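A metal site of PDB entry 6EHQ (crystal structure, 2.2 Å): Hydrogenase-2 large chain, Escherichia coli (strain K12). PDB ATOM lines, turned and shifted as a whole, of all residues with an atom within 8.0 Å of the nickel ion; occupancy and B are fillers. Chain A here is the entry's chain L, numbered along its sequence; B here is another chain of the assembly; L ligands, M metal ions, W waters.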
ATOM      1  N   GLU A  14       7.137 -21.592   7.647  1.00  0.00           N
ATOM      2  CA  GLU A  14       6.477 -21.680   8.921  1.00  0.00           C
ATOM      3  C   GLU A  14       7.343 -20.856   9.880  1.00  0.00           C
ATOM      4  O   GLU A  14       8.539 -21.100   9.992  1.00  0.00           O
ATOM      5  CB  GLU A  14       6.363 -23.133   9.388  1.00  0.00           C
ATOM      6  CG  GLU A  14       5.523 -23.294  10.643  1.00  0.00           C
ATOM      7  CD  GLU A  14       6.092 -22.565  11.883  1.00  0.00           C
ATOM      8  OE1 GLU A  14       7.332 -22.568  12.046  1.00  0.00           O
ATOM      9  OE2 GLU A  14       5.315 -21.995  12.686  1.00  0.00           O
ATOM     10  N   GLY A  15       6.735 -19.915  10.569  1.00  0.00           N
ATOM     11  CA  GLY A  15       7.343 -19.353  11.751  1.00  0.00           C
ATOM     12  C   GLY A  15       8.199 -18.141  11.501  1.00  0.00           C
ATOM     13  O   GLY A  15       8.145 -17.546  10.438  1.00  0.00           O
ATOM     14  N   ARG A  39       9.414 -20.800  22.511  1.00  0.00           N
ATOM     15  CA  ARG A  39       8.355 -21.156  23.464  1.00  0.00           C
ATOM     16  C   ARG A  39       8.820 -21.970  24.667  1.00  0.00           C
ATOM     17  O   ARG A  39       8.188 -21.926  25.718  1.00  0.00           O
ATOM     18  CB  ARG A  39       7.232 -21.911  22.749  1.00  0.00           C
ATOM     19  CG  ARG A  39       6.338 -21.001  21.884  1.00  0.00           C
ATOM     20  CD  ARG A  39       5.491 -21.770  20.864  1.00  0.00           C
ATOM     21  NE  ARG A  39       6.312 -22.570  19.974  1.00  0.00           N
ATOM     22  CZ  ARG A  39       5.909 -23.650  19.321  1.00  0.00           C
ATOM     23  NH1 ARG A  39       4.665 -24.100  19.440  1.00  0.00           N
ATOM     24  NH2 ARG A  39       6.773 -24.322  18.536  1.00  0.00           N
ATOM     25  N   GLN A  58       3.535 -32.531  20.093  1.00  0.00           N
ATOM     26  CA  GLN A  58       2.950 -32.368  18.741  1.00  0.00           C
ATOM     27  C   GLN A  58       2.795 -30.891  18.381  1.00  0.00           C
ATOM     28  O   GLN A  58       2.898 -30.517  17.200  1.00  0.00           O
ATOM     29  CB  GLN A  58       1.580 -33.058  18.577  1.00  0.00           C
ATOM     30  CG  GLN A  58       1.167 -33.053  17.110  1.00  0.00           C
ATOM     31  CD  GLN A  58       0.024 -33.982  16.718  1.00  0.00           C
ATOM     32  OE1 GLN A  58      -0.124 -34.314  15.532  1.00  0.00           O
ATOM     33  NE2 GLN A  58      -0.827 -34.350  17.684  1.00  0.00           N
ATOM     34  N   ILE A  60       4.795 -28.495  18.879  1.00  0.00           N
ATOM     35  CA  ILE A  60       5.970 -27.854  18.341  1.00  0.00           C
ATOM     36  C   ILE A  60       5.639 -27.237  16.985  1.00  0.00           C
ATOM     37  O   ILE A  60       6.047 -26.094  16.716  1.00  0.00           O
ATOM     38  CB  ILE A  60       7.130 -28.839  18.249  1.00  0.00           C
ATOM     39  CG1 ILE A  60       7.680 -29.088  19.682  1.00  0.00           C
ATOM     40  CG2 ILE A  60       8.199 -28.281  17.332  1.00  0.00           C
ATOM     41  CD1 ILE A  60       8.730 -30.210  19.789  1.00  0.00           C
ATOM     42  N   CYS A  61       4.877 -27.960  16.154  1.00  0.00           N
ATOM     43  CA  CYS A  61       4.548 -27.466  14.821  1.00  0.00           C
ATOM     44  C   CYS A  61       3.250 -28.053  14.253  1.00  0.00           C
ATOM     45  O   CYS A  61       3.009 -29.258  14.390  1.00  0.00           O
ATOM     46  CB  CYS A  61       5.699 -27.787  13.878  1.00  0.00           C
ATOM     47  SG  CYS A  61       5.555 -26.909  12.333  1.00  0.00           S
ATOM     48  N   GLY A  62       2.453 -27.193  13.606  1.00  0.00           N
ATOM     49  CA  GLY A  62       1.211 -27.607  12.945  1.00  0.00           C
ATOM     50  C   GLY A  62       1.350 -27.815  11.438  1.00  0.00           C
ATOM     51  O   GLY A  62       0.433 -28.353  10.805  1.00  0.00           O
ATOM     52  N   VAL A  63       2.460 -27.347  10.854  1.00  0.00           N
ATOM     53  CA  VAL A  63       2.758 -27.571   9.440  1.00  0.00           C
ATOM     54  C   VAL A  63       3.188 -29.011   9.262  1.00  0.00           C
ATOM     55  O   VAL A  63       2.610 -29.727   8.493  1.00  0.00           O
ATOM     56  CB  VAL A  63       3.812 -26.578   8.915  1.00  0.00           C
ATOM     57  CG1 VAL A  63       4.272 -26.935   7.514  1.00  0.00           C
ATOM     58  CG2 VAL A  63       3.223 -25.185   8.916  1.00  0.00           C
ATOM     59  N   CYS A  64       4.208 -29.437  10.019  1.00  0.00           N
ATOM     60  CA  CYS A  64       4.623 -30.825  10.077  1.00  0.00           C
ATOM     61  C   CYS A  64       3.943 -31.441  11.281  1.00  0.00           C
ATOM     62  O   CYS A  64       4.572 -32.012  12.190  1.00  0.00           O
ATOM     63  CB  CYS A  64       6.151 -30.956  10.182  1.00  0.00           C
ATOM     64  SG  CYS A  64       6.880 -30.225  11.688  1.00  0.00           S
ATOM     65  N   THR A  65       2.630 -31.323  11.306  1.00  0.00           N
ATOM     66  CA  THR A  65       1.827 -32.077  12.253  1.00  0.00           C
ATOM     67  C   THR A  65       2.041 -33.596  12.003  1.00  0.00           C
ATOM     68  O   THR A  65       2.531 -34.006  10.948  1.00  0.00           O
ATOM     69  CB  THR A  65       0.365 -31.597  12.223  1.00  0.00           C
ATOM     70  OG1 THR A  65      -0.334 -32.130  13.340  1.00  0.00           O
ATOM     71  CG2 THR A  65      -0.337 -31.979  10.970  1.00  0.00           C
ATOM     72  N   THR A  67       4.438 -35.380  13.004  1.00  0.00           N
ATOM     73  CA  THR A  67       5.835 -35.805  13.110  1.00  0.00           C
ATOM     74  C   THR A  67       6.348 -35.850  14.545  1.00  0.00           C
ATOM     75  O   THR A  67       6.900 -36.820  14.981  1.00  0.00           O
ATOM     76  CB  THR A  67       6.772 -34.891  12.298  1.00  0.00           C
ATOM     77  OG1 THR A  67       6.690 -33.561  12.785  1.00  0.00           O
ATOM     78  CG2 THR A  67       6.441 -34.926  10.847  1.00  0.00           C
ATOM     79  N   HIS A  68       6.152 -34.781  15.273  1.00  0.00           N
ATOM     80  CA  HIS A  68       6.564 -34.740  16.685  1.00  0.00           C
ATOM     81  C   HIS A  68       5.783 -35.704  17.583  1.00  0.00           C
ATOM     82  O   HIS A  68       6.337 -36.258  18.549  1.00  0.00           O
ATOM     83  CB  HIS A  68       6.529 -33.301  17.223  1.00  0.00           C
ATOM     84  CG  HIS A  68       7.491 -32.401  16.521  1.00  0.00           C
ATOM     85  ND1 HIS A  68       8.846 -32.451  16.749  1.00  0.00           N
ATOM     86  CD2 HIS A  68       7.294 -31.479  15.567  1.00  0.00           C
ATOM     87  CE1 HIS A  68       9.436 -31.582  15.961  1.00  0.00           C
ATOM     88  NE2 HIS A  68       8.513 -30.967  15.240  1.00  0.00           N
ATOM     89  N   HIS A  99       0.382 -37.341   5.291  1.00  0.00           N
ATOM     90  CA  HIS A  99       0.773 -36.028   5.738  1.00  0.00           C
ATOM     91  C   HIS A  99       1.900 -35.422   4.887  1.00  0.00           C
ATOM     92  O   HIS A  99       1.803 -34.258   4.450  1.00  0.00           O
ATOM     93  CB  HIS A  99       1.224 -36.003   7.189  1.00  0.00           C
ATOM     94  CG  HIS A  99       1.749 -34.658   7.541  1.00  0.00           C
ATOM     95  ND1 HIS A  99       0.913 -33.625   7.867  1.00  0.00           N
ATOM     96  CD2 HIS A  99       2.992 -34.130   7.423  1.00  0.00           C
ATOM     97  CE1 HIS A  99       1.626 -32.527   8.010  1.00  0.00           C
ATOM     98  NE2 HIS A  99       2.897 -32.801   7.749  1.00  0.00           N
ATOM     99  N   ASP A 103       2.254 -31.918   2.707  1.00  0.00           N
ATOM    100  CA  ASP A 103       3.258 -30.968   3.138  1.00  0.00           C
ATOM    101  C   ASP A 103       4.153 -30.583   1.956  1.00  0.00           C
ATOM    102  O   ASP A 103       4.331 -29.382   1.674  1.00  0.00           O
ATOM    103  CB  ASP A 103       4.034 -31.621   4.295  1.00  0.00           C
ATOM    104  CG  ASP A 103       4.836 -30.658   5.155  1.00  0.00           C
ATOM    105  OD1 ASP A 103       5.383 -29.639   4.589  1.00  0.00           O
ATOM    106  OD2 ASP A 103       5.000 -30.984   6.375  1.00  0.00           O
ATOM    107  N   ALA A 477      11.163 -37.005   8.839  1.00  0.00           N
ATOM    108  CA  ALA A 477      10.094 -36.023   8.641  1.00  0.00           C
ATOM    109  C   ALA A 477      10.207 -35.406   7.271  1.00  0.00           C
ATOM    110  O   ALA A 477      11.222 -35.589   6.597  1.00  0.00           O
ATOM    111  CB  ALA A 477      10.202 -34.920   9.710  1.00  0.00           C
ATOM    112  N   PRO A 478       9.202 -34.608   6.871  1.00  0.00           N
ATOM    113  CA  PRO A 478       9.264 -33.940   5.579  1.00  0.00           C
ATOM    114  C   PRO A 478      10.523 -33.090   5.318  1.00  0.00           C
ATOM    115  O   PRO A 478      10.999 -33.039   4.188  1.00  0.00           O
ATOM    116  CB  PRO A 478       8.021 -33.079   5.576  1.00  0.00           C
ATOM    117  CG  PRO A 478       7.061 -33.870   6.360  1.00  0.00           C
ATOM    118  CD  PRO A 478       7.860 -34.477   7.457  1.00  0.00           C
ATOM    119  N   ARG A 479      11.066 -32.489   6.374  1.00  0.00           N
ATOM    120  CA  ARG A 479      12.197 -31.617   6.281  1.00  0.00           C
ATOM    121  C   ARG A 479      13.464 -32.324   6.704  1.00  0.00           C
ATOM    122  O   ARG A 479      14.540 -31.700   6.639  1.00  0.00           O
ATOM    123  CB  ARG A 479      11.942 -30.346   7.109  1.00  0.00           C
ATOM    124  CG  ARG A 479      10.897 -29.481   6.437  1.00  0.00           C
ATOM    125  CD  ARG A 479      10.185 -28.542   7.391  1.00  0.00           C
ATOM    126  NE  ARG A 479       9.113 -27.865   6.649  1.00  0.00           N
ATOM    127  CZ  ARG A 479       7.887 -28.355   6.505  1.00  0.00           C
ATOM    128  NH1 ARG A 479       7.515 -29.459   7.147  1.00  0.00           N
ATOM    129  NH2 ARG A 479       7.013 -27.704   5.729  1.00  0.00           N
ATOM    130  N   VAL A 500      15.597 -31.195  15.725  1.00  0.00           N
ATOM    131  CA  VAL A 500      14.564 -31.155  14.692  1.00  0.00           C
ATOM    132  C   VAL A 500      15.244 -30.868  13.361  1.00  0.00           C
ATOM    133  O   VAL A 500      16.278 -30.222  13.352  1.00  0.00           O
ATOM    134  CB  VAL A 500      13.554 -30.098  15.120  1.00  0.00           C
ATOM    135  CG1 VAL A 500      12.365 -30.036  14.205  1.00  0.00           C
ATOM    136  CG2 VAL A 500      13.070 -30.406  16.543  1.00  0.00           C
ATOM    137  N   PRO A 501      14.700 -31.357  12.229  1.00  0.00           N
ATOM    138  CA  PRO A 501      15.501 -31.181  10.998  1.00  0.00           C
ATOM    139  C   PRO A 501      15.861 -29.748  10.647  1.00  0.00           C
ATOM    140  O   PRO A 501      16.986 -29.499  10.210  1.00  0.00           O
ATOM    141  CB  PRO A 501      14.650 -31.806   9.896  1.00  0.00           C
ATOM    142  CG  PRO A 501      13.385 -32.205  10.533  1.00  0.00           C
ATOM    143  CD  PRO A 501      13.579 -32.270  12.014  1.00  0.00           C
ATOM    144  N   SER A 502      14.948 -28.815  10.862  1.00  0.00           N
ATOM    145  CA  SER A 502      15.279 -27.420  10.581  1.00  0.00           C
ATOM    146  C   SER A 502      16.315 -26.871  11.585  1.00  0.00           C
ATOM    147  O   SER A 502      16.943 -25.876  11.279  1.00  0.00           O
ATOM    148  CB  SER A 502      14.050 -26.517  10.515  1.00  0.00           C
ATOM    149  OG  SER A 502      13.313 -26.786   9.345  1.00  0.00           O
ATOM    150  N   ASP A 544      12.786 -25.592   2.864  1.00  0.00           N
ATOM    151  CA  ASP A 544      11.466 -25.697   3.501  1.00  0.00           C
ATOM    152  C   ASP A 544      11.583 -25.357   5.027  1.00  0.00           C
ATOM    153  O   ASP A 544      11.283 -26.213   5.897  1.00  0.00           O
ATOM    154  CB  ASP A 544      10.970 -27.108   3.220  1.00  0.00           C
ATOM    155  CG  ASP A 544       9.562 -27.371   3.692  1.00  0.00           C
ATOM    156  OD1 ASP A 544       8.859 -26.446   4.142  1.00  0.00           O
ATOM    157  OD2 ASP A 544       9.197 -28.572   3.618  1.00  0.00           O
ATOM    158  N   PRO A 545      12.049 -24.138   5.353  1.00  0.00           N
ATOM    159  CA  PRO A 545      12.253 -23.786   6.747  1.00  0.00           C
ATOM    160  C   PRO A 545      10.987 -23.859   7.583  1.00  0.00           C
ATOM    161  O   PRO A 545       9.924 -23.420   7.131  1.00  0.00           O
ATOM    162  CB  PRO A 545      12.725 -22.320   6.694  1.00  0.00           C
ATOM    163  CG  PRO A 545      13.230 -22.137   5.341  1.00  0.00           C
ATOM    164  CD  PRO A 545      12.392 -23.017   4.474  1.00  0.00           C
ATOM    165  N   CYS A 546      11.149 -24.374   8.794  1.00  0.00           N
ATOM    166  CA  CYS A 546      10.101 -24.349   9.769  1.00  0.00           C
ATOM    167  C   CYS A 546      10.733 -23.935  11.081  1.00  0.00           C
ATOM    168  O   CYS A 546      11.377 -24.758  11.754  1.00  0.00           O
ATOM    169  CB  CYS A 546       9.424 -25.726   9.895  1.00  0.00           C
ATOM    170  SG  CYS A 546       8.048 -25.697  11.074  1.00  0.00           S
ATOM    171  N   MET A 547      10.539 -22.688  11.471  1.00  0.00           N
ATOM    172  CA  MET A 547      11.200 -22.146  12.665  1.00  0.00           C
ATOM    173  C   MET A 547      10.591 -22.532  13.988  1.00  0.00           C
ATOM    174  O   MET A 547      11.304 -22.579  14.985  1.00  0.00           O
ATOM    175  CB  MET A 547      11.336 -20.638  12.558  1.00  0.00           C
ATOM    176  CG  MET A 547      12.088 -20.252  11.285  1.00  0.00           C
ATOM    177  SD  MET A 547      13.574 -21.230  10.916  1.00  0.00           S
ATOM    178  CE  MET A 547      14.576 -20.709  12.315  1.00  0.00           C
ATOM    179  N   ALA A 548       9.300 -22.836  14.014  1.00  0.00           N
ATOM    180  CA  ALA A 548       8.693 -23.406  15.213  1.00  0.00           C
ATOM    181  C   ALA A 548       9.339 -24.735  15.491  1.00  0.00           C
ATOM    182  O   ALA A 548       9.673 -25.011  16.619  1.00  0.00           O
ATOM    183  CB  ALA A 548       7.190 -23.572  15.067  1.00  0.00           C
ATOM    184  N   CYS A 549       9.552 -25.532  14.454  1.00  0.00           N
ATOM    185  CA  CYS A 549      10.350 -26.751  14.550  1.00  0.00           C
ATOM    186  C   CYS A 549      11.790 -26.547  15.022  1.00  0.00           C
ATOM    187  O   CYS A 549      12.273 -27.232  15.936  1.00  0.00           O
ATOM    188  CB  CYS A 549      10.342 -27.477  13.223  1.00  0.00           C
ATOM    189  SG  CYS A 549       8.965 -28.636  13.076  1.00  0.00           S
ATOM    190  N   ALA A 550      12.469 -25.617  14.362  1.00  0.00           N
ATOM    191  CA  ALA A 550      13.889 -25.392  14.569  1.00  0.00           C
ATOM    192  C   ALA A 550      14.180 -25.022  16.021  1.00  0.00           C
ATOM    193  O   ALA A 550      15.164 -25.492  16.573  1.00  0.00           O
ATOM    194  CB  ALA A 550      14.391 -24.283  13.648  1.00  0.00           C
ATOM    195  N   CYS B  23       2.180 -22.382  16.368  1.00  0.00           N
ATOM    196  CA  CYS B  23       2.759 -23.548  15.698  1.00  0.00           C
ATOM    197  C   CYS B  23       2.376 -23.572  14.214  1.00  0.00           C
ATOM    198  O   CYS B  23       2.859 -24.427  13.473  1.00  0.00           O
ATOM    199  CB  CYS B  23       2.305 -24.848  16.402  1.00  0.00           C
ATOM    200  SG  CYS B  23       0.635 -25.451  15.992  1.00  0.00           S
ATOM    201  N   THR B  24       1.481 -22.645  13.824  1.00  0.00           N
ATOM    202  CA  THR B  24       0.951 -22.478  12.477  1.00  0.00           C
ATOM    203  C   THR B  24      -0.210 -23.451  12.157  1.00  0.00           C
ATOM    204  O   THR B  24      -0.771 -23.417  11.074  1.00  0.00           O
ATOM    205  CB  THR B  24       2.063 -22.436  11.394  1.00  0.00           C
ATOM    206  OG1 THR B  24       2.993 -21.407  11.733  1.00  0.00           O
ATOM    207  CG2 THR B  24       1.508 -22.102   9.993  1.00  0.00           C
HETATM  208 FE1  LIG L   1       9.173 -30.049  11.151  1.00  0.00          FE
HETATM  209  C1  LIG L   1      10.833 -29.437  10.752  1.00  0.00           C
HETATM  210  N1  LIG L   1      11.894 -29.060  10.559  1.00  0.00           N
HETATM  211  C2  LIG L   1       9.191 -31.158   9.695  1.00  0.00           C
HETATM  212  N2  LIG L   1       9.202 -31.843   8.758  1.00  0.00           N
HETATM  213  C3  LIG L   1       9.743 -31.491  12.092  1.00  0.00           C
HETATM  214  O1  LIG L   1      10.094 -32.395  12.651  1.00  0.00           O
HETATM  215 NI    NI M   1       7.330 -27.764  11.371  1.00  0.00          NI
HETATM  216  O   HOH W   1       8.248 -28.550  10.089  1.00  0.00           O
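A nitrogen (N2) of the ligand sits at hydrogen-bond distance from the guanidinium group (NH1) of Arg 479, at 3.3 Å. NE2 of His 68 lies within hydrogen-bond range of O1 of the ligand, at 3.4 Å. N1 of the ligand lies within hydrogen-bond range of N of Ser 502, 3.1 Å away. SG of Cys 64 is bound to FE1 of the ligand (2.4 Å). N of Arg 479 is in hydrogen-bond range of N2 of the ligand (3.1 Å). An iron atom (FE1) of the ligand is bound by the side-chain sulfur of Cys 549, 2.4 Å away. OG of Ser 502 sits at hydrogen-bond distance from N1 of the ligand, at 2.9 Å.
OE1 of Glu 14 lies close to SG of Cys 546, 3.4 Å away. SG of Cys 61 sits close to N of Val 63, 3.5 Å away. The side-chain sulfur (SG) of Cys 549 sits close to a ring nitrogen (NE2) of His 68 (3.2 Å). N of Cys 546 is in hydrogen-bond range of OG of Ser 502. The backbone carbonyl oxygen of Cys 64 sits at hydrogen-bond distance from the side-chain hydroxyl of Thr 67 (2.7 Å).
The nickel ion is bound by water W1 (1.8 Å). SG of Cys 61 is bound to the nickel ion. SG of Cys 546 binds the nickel ion, at 2.2 Å. SG of Cys 549 binds the nickel ion. The nickel ion is bound by SG of Cys 64 (2.5 Å). The nickel ion has five donor atoms within binding distance.
Four residues have an atom within 4 Å of the nickel ion: Cys 61, Cys 64, Cys 546 and Cys 549.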
